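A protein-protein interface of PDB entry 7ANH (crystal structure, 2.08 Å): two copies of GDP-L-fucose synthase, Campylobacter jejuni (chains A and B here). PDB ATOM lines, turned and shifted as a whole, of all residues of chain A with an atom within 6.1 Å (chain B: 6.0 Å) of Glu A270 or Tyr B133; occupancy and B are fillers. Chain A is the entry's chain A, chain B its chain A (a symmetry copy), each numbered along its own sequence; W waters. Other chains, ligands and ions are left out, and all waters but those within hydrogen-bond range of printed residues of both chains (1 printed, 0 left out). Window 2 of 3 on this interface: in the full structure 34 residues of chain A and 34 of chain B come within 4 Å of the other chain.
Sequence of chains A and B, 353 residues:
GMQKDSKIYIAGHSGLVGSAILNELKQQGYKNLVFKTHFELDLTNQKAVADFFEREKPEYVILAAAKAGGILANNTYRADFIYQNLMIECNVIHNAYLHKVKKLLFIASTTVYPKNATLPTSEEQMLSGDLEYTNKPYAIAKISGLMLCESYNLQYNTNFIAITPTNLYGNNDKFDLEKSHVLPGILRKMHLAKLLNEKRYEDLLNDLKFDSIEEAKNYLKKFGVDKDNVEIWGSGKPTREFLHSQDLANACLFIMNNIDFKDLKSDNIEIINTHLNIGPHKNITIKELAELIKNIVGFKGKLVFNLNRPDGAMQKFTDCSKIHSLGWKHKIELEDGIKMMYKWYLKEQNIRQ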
ATOM      1  N   LEU A 154      13.737   3.555  14.425  1.00  0.00           N
ATOM      2  CA  LEU A 154      12.467   2.854  14.227  1.00  0.00           C
ATOM      3  C   LEU A 154      12.023   2.046  15.464  1.00  0.00           C
ATOM      4  O   LEU A 154      10.861   2.117  15.816  1.00  0.00           O
ATOM      5  CB  LEU A 154      12.451   2.023  12.956  1.00  0.00           C
ATOM      6  CG  LEU A 154      12.410   2.791  11.641  1.00  0.00           C
ATOM      7  CD1 LEU A 154      12.739   1.859  10.500  1.00  0.00           C
ATOM      8  CD2 LEU A 154      11.054   3.468  11.412  1.00  0.00           C
ATOM      9  N   SER A 266       8.943   8.830   5.435  1.00  0.00           N
ATOM     10  CA  SER A 266       7.862   9.270   4.520  1.00  0.00           C
ATOM     11  C   SER A 266       6.456   8.758   4.888  1.00  0.00           C
ATOM     12  O   SER A 266       5.847   7.956   4.171  1.00  0.00           O
ATOM     13  CB  SER A 266       8.241   8.927   3.093  1.00  0.00           C
ATOM     14  OG  SER A 266       8.411   7.540   2.985  1.00  0.00           O
ATOM     15  N   ILE A 269       5.339   3.045   4.318  1.00  0.00           N
ATOM     16  CA  ILE A 269       5.424   2.330   5.621  1.00  0.00           C
ATOM     17  C   ILE A 269       6.675   1.459   5.810  1.00  0.00           C
ATOM     18  O   ILE A 269       6.919   0.974   6.911  1.00  0.00           O
ATOM     19  CB  ILE A 269       4.229   1.372   5.882  1.00  0.00           C
ATOM     20  CG1 ILE A 269       4.300   0.135   4.936  1.00  0.00           C
ATOM     21  CG2 ILE A 269       2.909   2.147   5.851  1.00  0.00           C
ATOM     22  CD1 ILE A 269       2.994  -0.622   4.760  1.00  0.00           C
ATOM     23  N   GLU A 270       7.409   1.202   4.737  1.00  0.00           N
ATOM     24  CA  GLU A 270       8.721   0.576   4.846  1.00  0.00           C
ATOM     25  C   GLU A 270       9.755   1.690   4.827  1.00  0.00           C
ATOM     26  O   GLU A 270      10.014   2.280   3.780  1.00  0.00           O
ATOM     27  CB  GLU A 270       8.931  -0.408   3.714  1.00  0.00           C
ATOM     28  CG  GLU A 270       8.120  -1.661   3.961  1.00  0.00           C
ATOM     29  CD  GLU A 270       8.092  -2.581   2.778  1.00  0.00           C
ATOM     30  OE1 GLU A 270       8.828  -2.324   1.782  1.00  0.00           O
ATOM     31  OE2 GLU A 270       7.304  -3.548   2.862  1.00  0.00           O
ATOM     32  N   ILE A 271      10.299   2.005   5.991  1.00  0.00           N
ATOM     33  CA  ILE A 271      11.211   3.125   6.126  1.00  0.00           C
ATOM     34  C   ILE A 271      12.671   2.663   5.962  1.00  0.00           C
ATOM     35  O   ILE A 271      13.217   1.994   6.856  1.00  0.00           O
ATOM     36  CB  ILE A 271      10.993   3.867   7.440  1.00  0.00           C
ATOM     37  CG1 ILE A 271       9.611   4.525   7.411  1.00  0.00           C
ATOM     38  CG2 ILE A 271      12.066   4.941   7.654  1.00  0.00           C
ATOM     39  CD1 ILE A 271       9.009   4.644   8.741  1.00  0.00           C
ATOM     40  N   ILE A 272      13.258   3.053   4.815  1.00  0.00           N
ATOM     41  CA  ILE A 272      14.680   2.786   4.443  1.00  0.00           C
ATOM     42  C   ILE A 272      15.332   4.052   3.890  1.00  0.00           C
ATOM     43  O   ILE A 272      14.666   4.996   3.458  1.00  0.00           O
ATOM     44  CB  ILE A 272      14.825   1.671   3.367  1.00  0.00           C
ATOM     45  CG1 ILE A 272      14.121   2.031   2.053  1.00  0.00           C
ATOM     46  CG2 ILE A 272      14.222   0.351   3.856  1.00  0.00           C
ATOM     47  CD1 ILE A 272      14.267   0.954   0.977  1.00  0.00           C
ATOM     48  N   ASN B  75      10.625  -7.270  12.236  1.00  0.00           N
ATOM     49  CA  ASN B  75      10.060  -5.997  11.878  1.00  0.00           C
ATOM     50  C   ASN B  75       9.747  -5.146  13.095  1.00  0.00           C
ATOM     51  O   ASN B  75       9.589  -3.963  12.982  1.00  0.00           O
ATOM     52  CB  ASN B  75       8.809  -6.207  11.030  1.00  0.00           C
ATOM     53  CG  ASN B  75       8.530  -5.038  10.130  1.00  0.00           C
ATOM     54  OD1 ASN B  75       9.373  -4.149   9.951  1.00  0.00           O
ATOM     55  ND2 ASN B  75       7.345  -5.021   9.549  1.00  0.00           N
ATOM     56  N   ARG B  78      14.032  -4.174  15.376  1.00  0.00           N
ATOM     57  CA  ARG B  78      14.998  -3.965  14.297  1.00  0.00           C
ATOM     58  C   ARG B  78      16.383  -3.632  14.867  1.00  0.00           C
ATOM     59  O   ARG B  78      17.373  -4.204  14.436  1.00  0.00           O
ATOM     60  CB  ARG B  78      14.484  -2.906  13.341  1.00  0.00           C
ATOM     61  CG  ARG B  78      13.169  -3.336  12.716  1.00  0.00           C
ATOM     62  CD  ARG B  78      12.678  -2.331  11.725  1.00  0.00           C
ATOM     63  NE  ARG B  78      13.470  -2.207  10.499  1.00  0.00           N
ATOM     64  CZ  ARG B  78      13.399  -3.027   9.448  1.00  0.00           C
ATOM     65  NH1 ARG B  78      12.631  -4.116   9.441  1.00  0.00           N
ATOM     66  NH2 ARG B  78      14.110  -2.751   8.379  1.00  0.00           N
ATOM     67  N   LYS B 115      16.390  -9.635  -2.862  1.00  0.00           N
ATOM     68  CA  LYS B 115      15.014 -10.052  -2.976  1.00  0.00           C
ATOM     69  C   LYS B 115      14.641 -10.369  -4.459  1.00  0.00           C
ATOM     70  O   LYS B 115      13.871 -11.269  -4.701  1.00  0.00           O
ATOM     71  CB  LYS B 115      14.131  -8.952  -2.394  1.00  0.00           C
ATOM     72  CG  LYS B 115      12.635  -9.253  -2.401  1.00  0.00           C
ATOM     73  CD  LYS B 115      11.815  -7.965  -2.382  1.00  0.00           C
ATOM     74  CE  LYS B 115      10.331  -8.252  -2.173  1.00  0.00           C
ATOM     75  NZ  LYS B 115       9.662  -7.196  -1.354  1.00  0.00           N
ATOM     76  N   LEU B 131      17.879  -5.654  -0.444  1.00  0.00           N
ATOM     77  CA  LEU B 131      17.307  -6.636   0.431  1.00  0.00           C
ATOM     78  C   LEU B 131      15.849  -6.349   0.731  1.00  0.00           C
ATOM     79  O   LEU B 131      15.417  -5.217   0.645  1.00  0.00           O
ATOM     80  CB  LEU B 131      18.097  -6.682   1.748  1.00  0.00           C
ATOM     81  CG  LEU B 131      19.577  -7.059   1.539  1.00  0.00           C
ATOM     82  CD1 LEU B 131      20.356  -6.758   2.807  1.00  0.00           C
ATOM     83  CD2 LEU B 131      19.765  -8.494   1.026  1.00  0.00           C
ATOM     84  N   GLU B 132      15.135  -7.411   1.111  1.00  0.00           N
ATOM     85  CA  GLU B 132      13.775  -7.374   1.668  1.00  0.00           C
ATOM     86  C   GLU B 132      13.819  -6.481   2.886  1.00  0.00           C
ATOM     87  O   GLU B 132      14.761  -6.514   3.695  1.00  0.00           O
ATOM     88  CB  GLU B 132      13.305  -8.826   1.987  1.00  0.00           C
ATOM     89  CG  GLU B 132      12.118  -9.053   2.938  1.00  0.00           C
ATOM     90  CD  GLU B 132      10.895  -8.199   2.605  1.00  0.00           C
ATOM     91  OE1 GLU B 132      10.593  -8.042   1.383  1.00  0.00           O
ATOM     92  OE2 GLU B 132      10.293  -7.633   3.574  1.00  0.00           O
ATOM     93  N   TYR B 133      12.784  -5.646   2.986  1.00  0.00           N
ATOM     94  CA  TYR B 133      12.661  -4.691   4.056  1.00  0.00           C
ATOM     95  C   TYR B 133      12.575  -5.343   5.424  1.00  0.00           C
ATOM     96  O   TYR B 133      13.204  -4.878   6.359  1.00  0.00           O
ATOM     97  CB  TYR B 133      11.424  -3.775   3.835  1.00  0.00           C
ATOM     98  CG  TYR B 133      11.140  -2.961   5.073  1.00  0.00           C
ATOM     99  CD1 TYR B 133      11.852  -1.789   5.320  1.00  0.00           C
ATOM    100  CD2 TYR B 133      10.200  -3.389   6.043  1.00  0.00           C
ATOM    101  CE1 TYR B 133      11.610  -1.043   6.454  1.00  0.00           C
ATOM    102  CE2 TYR B 133       9.966  -2.642   7.192  1.00  0.00           C
ATOM    103  CZ  TYR B 133      10.670  -1.474   7.385  1.00  0.00           C
ATOM    104  OH  TYR B 133      10.508  -0.721   8.508  1.00  0.00           O
ATOM    105  N   THR B 134      11.743  -6.372   5.568  1.00  0.00           N
ATOM    106  CA  THR B 134      11.341  -6.804   6.908  1.00  0.00           C
ATOM    107  C   THR B 134      12.447  -7.419   7.758  1.00  0.00           C
ATOM    108  O   THR B 134      12.396  -7.365   8.979  1.00  0.00           O
ATOM    109  CB  THR B 134      10.135  -7.757   6.891  1.00  0.00           C
ATOM    110  OG1 THR B 134      10.367  -8.807   5.960  1.00  0.00           O
ATOM    111  CG2 THR B 134       8.861  -7.015   6.497  1.00  0.00           C
ATOM    112  N   ASN B 135      13.436  -7.995   7.110  1.00  0.00           N
ATOM    113  CA  ASN B 135      14.564  -8.623   7.809  1.00  0.00           C
ATOM    114  C   ASN B 135      15.896  -7.923   7.494  1.00  0.00           C
ATOM    115  O   ASN B 135      16.966  -8.470   7.762  1.00  0.00           O
ATOM    116  CB  ASN B 135      14.655 -10.105   7.388  1.00  0.00           C
ATOM    117  CG  ASN B 135      14.846 -10.270   5.881  1.00  0.00           C
ATOM    118  OD1 ASN B 135      15.219  -9.315   5.138  1.00  0.00           O
ATOM    119  ND2 ASN B 135      14.586 -11.477   5.407  1.00  0.00           N
ATOM    120  N   LYS B 136      15.798  -6.718   6.914  1.00  0.00           N
ATOM    121  CA  LYS B 136      16.922  -5.964   6.459  1.00  0.00           C
ATOM    122  C   LYS B 136      17.993  -5.807   7.532  1.00  0.00           C
ATOM    123  O   LYS B 136      19.129  -5.993   7.250  1.00  0.00           O
ATOM    124  CB  LYS B 136      16.483  -4.627   5.858  1.00  0.00           C
ATOM    125  CG  LYS B 136      17.653  -3.937   5.230  1.00  0.00           C
ATOM    126  CD  LYS B 136      17.264  -2.754   4.397  1.00  0.00           C
ATOM    127  CE  LYS B 136      17.343  -3.075   2.939  1.00  0.00           C
ATOM    128  NZ  LYS B 136      16.880  -1.955   2.115  1.00  0.00           N
ATOM    129  N   PRO B 137      17.624  -5.569   8.786  1.00  0.00           N
ATOM    130  CA  PRO B 137      18.732  -5.402   9.730  1.00  0.00           C
ATOM    131  C   PRO B 137      19.508  -6.713  10.094  1.00  0.00           C
ATOM    132  O   PRO B 137      20.703  -6.684  10.305  1.00  0.00           O
ATOM    133  CB  PRO B 137      18.059  -4.778  10.968  1.00  0.00           C
ATOM    134  CG  PRO B 137      16.689  -4.354  10.527  1.00  0.00           C
ATOM    135  CD  PRO B 137      16.348  -5.044   9.292  1.00  0.00           C
HETATM  136  O   HOH W   1      15.075   0.046   7.898  1.00  0.00           O
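Of the 10 printed residues of chain B, 2 touch a printed residue of chain A. Printed residues of chain B that touch a printed residue of chain A: Tyr B133 and Lys B136. Along chain B the printed residues that touch a printed residue of chain A span positions 133 to 136. Of the 6 printed residues of chain A, 4 touch a printed residue of chain B. Among the printed residues, 5 pairs touch across the chains.
Glu A270 touches just one residue of chain B: Tyr B133 (3.4 Å). Tyr B133 touches four residues of chain A. Of the printed residues of chain B, Ile A271 touches Tyr B133. Of the printed residues of chain B, Leu A154 touches Tyr B133. The nearest residue of chain A that does not touch Tyr B133 is Ile A269 (4.3 Å).
CD1 of Leu A154 touches OH of Tyr B133 (3.9 Å). CD2 of Tyr B133 touches CG of Glu A270, 3.4 Å away. Tyr B133 touches Ile A271 (CE1 to N, 3.4 Å). Ile A272 touches Tyr B133 (CG2 to CD1, 3.5 Å). CG2 of Ile A272 touches NZ of Lys B136, 3.9 Å away.
Water W1 bridges O of Ile A271 (2.9 Å) and NH2 of Arg B78 (3.0 Å).
O of Tyr B133 sits at hydrogen-bond distance from NH2 of Arg B78, at 3.1 Å.
No position is printed for both chains.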
